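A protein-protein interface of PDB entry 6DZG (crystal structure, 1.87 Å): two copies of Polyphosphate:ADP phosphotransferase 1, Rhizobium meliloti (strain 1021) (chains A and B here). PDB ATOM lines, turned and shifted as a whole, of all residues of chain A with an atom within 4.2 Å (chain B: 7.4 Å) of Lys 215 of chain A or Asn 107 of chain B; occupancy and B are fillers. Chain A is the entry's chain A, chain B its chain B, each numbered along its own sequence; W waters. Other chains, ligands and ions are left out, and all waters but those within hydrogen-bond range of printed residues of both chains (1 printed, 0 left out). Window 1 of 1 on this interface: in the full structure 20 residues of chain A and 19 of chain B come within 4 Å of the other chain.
The side-chain amide oxygen (OD1) of Asn 107 of chain B sits close to the backbone carbonyl oxygen (O) of Leu 214 of chain A, at 3.3 Å. The backbone carbonyl oxygen (O) of Asn 107 of chain B lies within hydrogen-bond range of the indole nitrogen (NE1) of Trp 217 of chain A (3.2 Å).
O of Arg 209 of chain A sits close to N of Ile 216 of chain A, at 3.3 Å. The side-chain carboxylate (OD1) of Asp 212 of chain A sits close to the backbone NH (N) of Leu 214 of chain A. O of Leu 214 of chain A is in hydrogen-bond range of NE1 of Trp 217 of chain A, at 3.0 Å. The backbone carbonyl oxygen of Ala 103 of chain B sits at hydrogen-bond distance from the side-chain amide nitrogen of Gln 68 of chain B, 2.9 Å away. The side-chain amide oxygen (OE1) of Gln 68 of chain B sits at hydrogen-bond distance from the side-chain amide nitrogen (ND2) of Asn 107 of chain B, 3.3 Å away. The side-chain amide oxygen (OE1) of Gln 75 of chain B lies within hydrogen-bond range of the backbone NH (N) of Asn 109 of chain B, 2.9 Å away.
Pro 213 of chain A touches Ile 69 of chain B. CG1 of Val 72 of chain B touches O of Pro 213 of chain A (3.7 Å). CD1 of Leu 214 of chain A touches N of Ile 69 of chain B, at 3.8 Å. O of Leu 214 of chain A touches CG2 of Val 72 of chain B, at 3.8 Å. Lys 215 of chain A touches Asn 107 of chain B (CD to OD1, 3.3 Å). Ile 216 of chain A touches Val 72 of chain B. Ile 216 of chain A touches Phe 76 of chain B. CD1 of Trp 217 of chain A touches CG2 of Val 72 of chain B (3.7 Å). Asn 109 of chain B touches Trp 217 of chain A (CA to CZ3, 3.6 Å). CZ3 of Trp 217 of chain A touches CD of Pro 110 of chain B (3.9 Å).
Of chain B, only Asn 107 (3.3 Å) comes within 4 Å of Lys 215 of chain A. Asn 107 of chain B touches just these residues of chain A: Leu 214 (3.3 Å), Lys 215 (3.3 Å) and Trp 217 (3.2 Å). Printed residues of chain A within 4 Å of Val 72 of chain B: Pro 213, Leu 214, Ile 216 and Trp 217. Printed residues of chain A within 4 Å of Gln 68 of chain B: Leu 214 (3.5 Å). The nearest residue of chain B that does not touch Lys 215 of chain A is Val 72 of chain B (5.3 Å). The nearest printed residue of chain A that does not touch Asn 107 of chain B is Lys 218 of chain A (4.8 Å).
Printed residues of chain B that touch a printed residue of chain A: Gln 68, Ile 69, Val 72, Phe 76, Asn 107, Met 108, Asn 109 and Pro 110. Along chain B the printed residues that touch a printed residue of chain A span positions 68 to 110. Among the printed residues, 14 pairs touch across the chains. Among the printed residues, no Asp or Glu carboxylate lies within 4 Å of a Lys or Arg side-chain nitrogen of the other chain.
No position is printed for both chains. Of the 14 pairs that touch across the chains among the printed residues, none has its exchanged pair printed and touching as well.
Water W1 lies within hydrogen-bond range of the backbone carbonyl oxygen (O) of Pro 213 of chain A (2.9 Å) and the backbone carbonyl oxygen (O) of Ile 69 of chain B (2.9 Å).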
ATOM      1  N   ARG A 209      21.493 -25.228  33.515  1.00  0.00           N
ATOM      2  CA  ARG A 209      20.855 -24.585  32.379  1.00  0.00           C
ATOM      3  C   ARG A 209      19.354 -24.480  32.573  1.00  0.00           C
ATOM      4  O   ARG A 209      18.763 -23.439  32.273  1.00  0.00           O
ATOM      5  CB  ARG A 209      21.183 -25.355  31.111  1.00  0.00           C
ATOM      6  CG  ARG A 209      22.657 -25.226  30.784  1.00  0.00           C
ATOM      7  CD  ARG A 209      23.119 -26.175  29.706  1.00  0.00           C
ATOM      8  NE  ARG A 209      24.540 -25.947  29.470  1.00  0.00           N
ATOM      9  CZ  ARG A 209      25.204 -26.359  28.393  1.00  0.00           C
ATOM     10  NH1 ARG A 209      24.587 -27.045  27.439  1.00  0.00           N
ATOM     11  NH2 ARG A 209      26.496 -26.078  28.282  1.00  0.00           N
ATOM     12  N   ASP A 212      18.447 -21.534  35.009  1.00  0.00           N
ATOM     13  CA  ASP A 212      19.004 -20.205  34.769  1.00  0.00           C
ATOM     14  C   ASP A 212      18.250 -19.592  33.601  1.00  0.00           C
ATOM     15  O   ASP A 212      18.395 -20.070  32.459  1.00  0.00           O
ATOM     16  CB  ASP A 212      20.502 -20.296  34.474  1.00  0.00           C
ATOM     17  CG  ASP A 212      21.168 -18.927  34.370  1.00  0.00           C
ATOM     18  OD1 ASP A 212      20.450 -17.908  34.412  1.00  0.00           O
ATOM     19  OD2 ASP A 212      22.413 -18.874  34.238  1.00  0.00           O
ATOM     20  N   PRO A 213      17.432 -18.558  33.820  1.00  0.00           N
ATOM     21  CA  PRO A 213      16.637 -17.998  32.707  1.00  0.00           C
ATOM     22  C   PRO A 213      17.485 -17.549  31.533  1.00  0.00           C
ATOM     23  O   PRO A 213      16.985 -17.492  30.402  1.00  0.00           O
ATOM     24  CB  PRO A 213      15.909 -16.814  33.356  1.00  0.00           C
ATOM     25  CG  PRO A 213      15.873 -17.157  34.821  1.00  0.00           C
ATOM     26  CD  PRO A 213      17.172 -17.864  35.092  1.00  0.00           C
ATOM     27  N   LEU A 214      18.762 -17.262  31.770  1.00  0.00           N
ATOM     28  CA  LEU A 214      19.676 -16.814  30.736  1.00  0.00           C
ATOM     29  C   LEU A 214      20.235 -17.962  29.912  1.00  0.00           C
ATOM     30  O   LEU A 214      20.665 -17.733  28.782  1.00  0.00           O
ATOM     31  CB  LEU A 214      20.830 -16.040  31.383  1.00  0.00           C
ATOM     32  CG  LEU A 214      21.810 -15.308  30.478  1.00  0.00           C
ATOM     33  CD1 LEU A 214      21.053 -14.270  29.668  1.00  0.00           C
ATOM     34  CD2 LEU A 214      22.899 -14.671  31.341  1.00  0.00           C
ATOM     35  N   LYS A 215      20.241 -19.184  30.451  1.00  0.00           N
ATOM     36  CA  LYS A 215      20.851 -20.321  29.778  1.00  0.00           C
ATOM     37  C   LYS A 215      19.861 -21.427  29.446  1.00  0.00           C
ATOM     38  O   LYS A 215      20.267 -22.449  28.880  1.00  0.00           O
ATOM     39  CB  LYS A 215      21.985 -20.909  30.632  1.00  0.00           C
ATOM     40  CG  LYS A 215      23.043 -19.912  31.055  1.00  0.00           C
ATOM     41  CD  LYS A 215      23.764 -19.338  29.869  1.00  0.00           C
ATOM     42  CE  LYS A 215      24.777 -18.306  30.317  1.00  0.00           C
ATOM     43  NZ  LYS A 215      25.478 -18.772  31.545  1.00  0.00           N
ATOM     44  N   ILE A 216      18.580 -21.262  29.783  1.00  0.00           N
ATOM     45  CA  ILE A 216      17.611 -22.312  29.503  1.00  0.00           C
ATOM     46  C   ILE A 216      17.488 -22.552  27.999  1.00  0.00           C
ATOM     47  O   ILE A 216      17.111 -23.654  27.584  1.00  0.00           O
ATOM     48  CB  ILE A 216      16.272 -21.955  30.186  1.00  0.00           C
ATOM     49  CG1 ILE A 216      15.318 -23.160  30.235  1.00  0.00           C
ATOM     50  CG2 ILE A 216      15.617 -20.759  29.532  1.00  0.00           C
ATOM     51  CD1 ILE A 216      13.991 -22.852  30.902  1.00  0.00           C
ATOM     52  N   TRP A 217      17.836 -21.565  27.159  1.00  0.00           N
ATOM     53  CA  TRP A 217      17.820 -21.801  25.714  1.00  0.00           C
ATOM     54  C   TRP A 217      18.742 -22.954  25.332  1.00  0.00           C
ATOM     55  O   TRP A 217      18.489 -23.650  24.340  1.00  0.00           O
ATOM     56  CB  TRP A 217      18.219 -20.535  24.944  1.00  0.00           C
ATOM     57  CG  TRP A 217      19.617 -20.055  25.208  1.00  0.00           C
ATOM     58  CD1 TRP A 217      20.014 -19.187  26.193  1.00  0.00           C
ATOM     59  CD2 TRP A 217      20.806 -20.409  24.484  1.00  0.00           C
ATOM     60  NE1 TRP A 217      21.379 -18.987  26.127  1.00  0.00           N
ATOM     61  CE2 TRP A 217      21.886 -19.726  25.090  1.00  0.00           C
ATOM     62  CE3 TRP A 217      21.064 -21.246  23.389  1.00  0.00           C
ATOM     63  CZ2 TRP A 217      23.203 -19.840  24.624  1.00  0.00           C
ATOM     64  CZ3 TRP A 217      22.374 -21.359  22.929  1.00  0.00           C
ATOM     65  CH2 TRP A 217      23.425 -20.660  23.550  1.00  0.00           C
ATOM     66  N   LYS A 218      19.794 -23.187  26.120  1.00  0.00           N
ATOM     67  CA  LYS A 218      20.757 -24.239  25.821  1.00  0.00           C
ATOM     68  C   LYS A 218      20.176 -25.640  25.962  1.00  0.00           C
ATOM     69  O   LYS A 218      20.829 -26.598  25.542  1.00  0.00           O
ATOM     70  CB  LYS A 218      21.978 -24.099  26.730  1.00  0.00           C
ATOM     71  CG  LYS A 218      22.834 -22.865  26.453  1.00  0.00           C
ATOM     72  CD  LYS A 218      24.033 -22.833  27.401  1.00  0.00           C
ATOM     73  CE  LYS A 218      24.977 -21.681  27.095  1.00  0.00           C
ATOM     74  NZ  LYS A 218      26.112 -21.681  28.057  1.00  0.00           N
ATOM     75  N   LEU B  64      22.330  -5.614  31.083  1.00  0.00           N
ATOM     76  CA  LEU B  64      22.401  -6.449  29.886  1.00  0.00           C
ATOM     77  C   LEU B  64      21.919  -7.865  30.178  1.00  0.00           C
ATOM     78  O   LEU B  64      21.214  -8.461  29.364  1.00  0.00           O
ATOM     79  CB  LEU B  64      23.830  -6.473  29.331  1.00  0.00           C
ATOM     80  CG  LEU B  64      24.089  -7.375  28.108  1.00  0.00           C
ATOM     81  CD1 LEU B  64      23.255  -6.967  26.914  1.00  0.00           C
ATOM     82  CD2 LEU B  64      25.558  -7.362  27.764  1.00  0.00           C
ATOM     83  N   THR B  65      22.293  -8.421  31.335  1.00  0.00           N
ATOM     84  CA  THR B  65      21.802  -9.748  31.708  1.00  0.00           C
ATOM     85  C   THR B  65      20.277  -9.793  31.697  1.00  0.00           C
ATOM     86  O   THR B  65      19.669 -10.719  31.140  1.00  0.00           O
ATOM     87  CB  THR B  65      22.332 -10.146  33.085  1.00  0.00           C
ATOM     88  OG1 THR B  65      23.738 -10.416  33.000  1.00  0.00           O
ATOM     89  CG2 THR B  65      21.611 -11.386  33.591  1.00  0.00           C
ATOM     90  N   GLN B  68      19.085  -9.739  28.034  1.00  0.00           N
ATOM     91  CA  GLN B  68      19.288 -11.015  27.353  1.00  0.00           C
ATOM     92  C   GLN B  68      18.323 -12.089  27.852  1.00  0.00           C
ATOM     93  O   GLN B  68      17.896 -12.949  27.072  1.00  0.00           O
ATOM     94  CB  GLN B  68      20.737 -11.474  27.529  1.00  0.00           C
ATOM     95  CG  GLN B  68      21.746 -10.569  26.846  1.00  0.00           C
ATOM     96  CD  GLN B  68      23.174 -11.014  27.080  1.00  0.00           C
ATOM     97  OE1 GLN B  68      23.467 -11.750  28.031  1.00  0.00           O
ATOM     98  NE2 GLN B  68      24.075 -10.573  26.213  1.00  0.00           N
ATOM     99  N   ILE B  69      17.971 -12.065  29.137  1.00  0.00           N
ATOM    100  CA  ILE B  69      16.916 -12.954  29.624  1.00  0.00           C
ATOM    101  C   ILE B  69      15.621 -12.714  28.857  1.00  0.00           C
ATOM    102  O   ILE B  69      14.900 -13.660  28.500  1.00  0.00           O
ATOM    103  CB  ILE B  69      16.715 -12.766  31.138  1.00  0.00           C
ATOM    104  CG1 ILE B  69      17.897 -13.369  31.912  1.00  0.00           C
ATOM    105  CG2 ILE B  69      15.388 -13.368  31.554  1.00  0.00           C
ATOM    106  CD1 ILE B  69      17.882 -13.081  33.415  1.00  0.00           C
ATOM    107  N   LEU B  71      15.538 -11.596  25.795  1.00  0.00           N
ATOM    108  CA  LEU B  71      15.738 -12.057  24.419  1.00  0.00           C
ATOM    109  C   LEU B  71      15.611 -13.575  24.296  1.00  0.00           C
ATOM    110  O   LEU B  71      15.277 -14.082  23.211  1.00  0.00           O
ATOM    111  CB  LEU B  71      17.097 -11.600  23.892  1.00  0.00           C
ATOM    112  CG  LEU B  71      17.268 -10.132  23.476  1.00  0.00           C
ATOM    113  CD1 LEU B  71      18.756  -9.823  23.348  1.00  0.00           C
ATOM    114  CD2 LEU B  71      16.545  -9.789  22.179  1.00  0.00           C
ATOM    115  N   VAL B  72      15.910 -14.312  25.373  1.00  0.00           N
ATOM    116  CA  VAL B  72      15.630 -15.748  25.419  1.00  0.00           C
ATOM    117  C   VAL B  72      14.137 -15.989  25.253  1.00  0.00           C
ATOM    118  O   VAL B  72      13.706 -16.870  24.493  1.00  0.00           O
ATOM    119  CB  VAL B  72      16.150 -16.363  26.737  1.00  0.00           C
ATOM    120  CG1 VAL B  72      15.587 -17.795  26.948  1.00  0.00           C
ATOM    121  CG2 VAL B  72      17.678 -16.380  26.767  1.00  0.00           C
ATOM    122  N   GLN B  75      13.235 -15.400  21.637  1.00  0.00           N
ATOM    123  CA  GLN B  75      13.570 -16.514  20.762  1.00  0.00           C
ATOM    124  C   GLN B  75      12.581 -17.653  20.918  1.00  0.00           C
ATOM    125  O   GLN B  75      12.147 -18.242  19.922  1.00  0.00           O
ATOM    126  CB  GLN B  75      14.987 -17.008  21.033  1.00  0.00           C
ATOM    127  CG  GLN B  75      16.003 -16.295  20.198  1.00  0.00           C
ATOM    128  CD  GLN B  75      17.104 -17.206  19.764  1.00  0.00           C
ATOM    129  OE1 GLN B  75      17.797 -17.796  20.599  1.00  0.00           O
ATOM    130  NE2 GLN B  75      17.270 -17.355  18.444  1.00  0.00           N
ATOM    131  N   PHE B  76      12.213 -17.980  22.159  1.00  0.00           N
ATOM    132  CA  PHE B  76      11.197 -19.006  22.383  1.00  0.00           C
ATOM    133  C   PHE B  76       9.894 -18.651  21.686  1.00  0.00           C
ATOM    134  O   PHE B  76       9.255 -19.510  21.067  1.00  0.00           O
ATOM    135  CB  PHE B  76      10.962 -19.196  23.880  1.00  0.00           C
ATOM    136  CG  PHE B  76      11.935 -20.127  24.524  1.00  0.00           C
ATOM    137  CD1 PHE B  76      12.158 -21.387  23.991  1.00  0.00           C
ATOM    138  CD2 PHE B  76      12.650 -19.740  25.649  1.00  0.00           C
ATOM    139  CE1 PHE B  76      13.066 -22.253  24.577  1.00  0.00           C
ATOM    140  CE2 PHE B  76      13.560 -20.599  26.234  1.00  0.00           C
ATOM    141  CZ  PHE B  76      13.773 -21.855  25.701  1.00  0.00           C
ATOM    142  N   HIS B 102      27.055  -8.697  19.081  1.00  0.00           N
ATOM    143  CA  HIS B 102      27.393  -9.751  20.037  1.00  0.00           C
ATOM    144  C   HIS B 102      26.556  -9.641  21.306  1.00  0.00           C
ATOM    145  O   HIS B 102      26.150 -10.661  21.876  1.00  0.00           O
ATOM    146  CB  HIS B 102      28.872  -9.740  20.405  1.00  0.00           C
ATOM    147  CG  HIS B 102      29.211 -10.730  21.477  1.00  0.00           C
ATOM    148  ND1 HIS B 102      29.022 -12.087  21.321  1.00  0.00           N
ATOM    149  CD2 HIS B 102      29.684 -10.560  22.736  1.00  0.00           C
ATOM    150  CE1 HIS B 102      29.387 -12.712  22.427  1.00  0.00           C
ATOM    151  NE2 HIS B 102      29.793 -11.809  23.300  1.00  0.00           N
ATOM    152  N   ALA B 103      26.298  -8.416  21.780  1.00  0.00           N
ATOM    153  CA  ALA B 103      25.453  -8.282  22.963  1.00  0.00           C
ATOM    154  C   ALA B 103      24.062  -8.848  22.713  1.00  0.00           C
ATOM    155  O   ALA B 103      23.437  -9.403  23.631  1.00  0.00           O
ATOM    156  CB  ALA B 103      25.379  -6.816  23.397  1.00  0.00           C
ATOM    157  N   THR B 104      23.566  -8.750  21.476  1.00  0.00           N
ATOM    158  CA  THR B 104      22.248  -9.302  21.184  1.00  0.00           C
ATOM    159  C   THR B 104      22.284 -10.824  21.120  1.00  0.00           C
ATOM    160  O   THR B 104      21.376 -11.482  21.639  1.00  0.00           O
ATOM    161  CB  THR B 104      21.695  -8.727  19.872  1.00  0.00           C
ATOM    162  OG1 THR B 104      21.570  -7.310  19.981  1.00  0.00           O
ATOM    163  CG2 THR B 104      20.323  -9.290  19.558  1.00  0.00           C
ATOM    164  N   THR B 105      23.320 -11.404  20.496  1.00  0.00           N
ATOM    165  CA  THR B 105      23.333 -12.836  20.203  1.00  0.00           C
ATOM    166  C   THR B 105      24.046 -13.685  21.242  1.00  0.00           C
ATOM    167  O   THR B 105      24.033 -14.908  21.111  1.00  0.00           O
ATOM    168  CB  THR B 105      23.977 -13.107  18.842  1.00  0.00           C
ATOM    169  OG1 THR B 105      25.358 -12.741  18.879  1.00  0.00           O
ATOM    170  CG2 THR B 105      23.271 -12.317  17.754  1.00  0.00           C
ATOM    171  N   ALA B 106      24.641 -13.085  22.280  1.00  0.00           N
ATOM    172  CA  ALA B 106      25.496 -13.845  23.190  1.00  0.00           C
ATOM    173  C   ALA B 106      24.780 -15.056  23.778  1.00  0.00           C
ATOM    174  O   ALA B 106      25.376 -16.127  23.935  1.00  0.00           O
ATOM    175  CB  ALA B 106      25.998 -12.938  24.321  1.00  0.00           C
ATOM    176  N   ASN B 107      23.519 -14.903  24.133  1.00  0.00           N
ATOM    177  CA  ASN B 107      22.758 -15.977  24.740  1.00  0.00           C
ATOM    178  C   ASN B 107      21.573 -16.333  23.874  1.00  0.00           C
ATOM    179  O   ASN B 107      20.457 -16.547  24.357  1.00  0.00           O
ATOM    180  CB  ASN B 107      22.318 -15.616  26.155  1.00  0.00           C
ATOM    181  CG  ASN B 107      23.378 -15.959  27.174  1.00  0.00           C
ATOM    182  OD1 ASN B 107      23.597 -17.137  27.481  1.00  0.00           O
ATOM    183  ND2 ASN B 107      24.068 -14.942  27.679  1.00  0.00           N
ATOM    184  N   MET B 108      21.814 -16.380  22.573  1.00  0.00           N
ATOM    185  CA  MET B 108      20.846 -16.896  21.628  1.00  0.00           C
ATOM    186  C   MET B 108      21.344 -18.181  20.980  1.00  0.00           C
ATOM    187  O   MET B 108      22.555 -18.417  20.889  1.00  0.00           O
ATOM    188  CB  MET B 108      20.557 -15.847  20.562  1.00  0.00           C
ATOM    189  CG  MET B 108      19.727 -14.707  21.087  1.00  0.00           C
ATOM    190  SD  MET B 108      19.379 -13.425  19.672  1.00  0.00           S
ATOM    191  CE  MET B 108      17.838 -12.539  20.460  1.00  0.00           C
ATOM    192  N   ASN B 109      20.396 -18.987  20.531  1.00  0.00           N
ATOM    193  CA  ASN B 109      20.677 -20.267  19.903  1.00  0.00           C
ATOM    194  C   ASN B 109      21.294 -20.025  18.531  1.00  0.00           C
ATOM    195  O   ASN B 109      20.607 -19.511  17.640  1.00  0.00           O
ATOM    196  CB  ASN B 109      19.384 -21.066  19.776  1.00  0.00           C
ATOM    197  CG  ASN B 109      19.621 -22.524  19.432  1.00  0.00           C
ATOM    198  OD1 ASN B 109      20.582 -22.874  18.741  1.00  0.00           O
ATOM    199  ND2 ASN B 109      18.742 -23.393  19.935  1.00  0.00           N
ATOM    200  N   PRO B 110      22.547 -20.417  18.295  1.00  0.00           N
ATOM    201  CA  PRO B 110      23.151 -20.156  16.979  1.00  0.00           C
ATOM    202  C   PRO B 110      22.451 -20.870  15.824  1.00  0.00           C
ATOM    203  O   PRO B 110      22.728 -20.541  14.671  1.00  0.00           O
ATOM    204  CB  PRO B 110      24.595 -20.649  17.149  1.00  0.00           C
ATOM    205  CG  PRO B 110      24.531 -21.642  18.272  1.00  0.00           C
ATOM    206  CD  PRO B 110      23.469 -21.128  19.203  1.00  0.00           C
HETATM  207  O   HOH W   1      14.448 -16.247  29.821  1.00  0.00           O
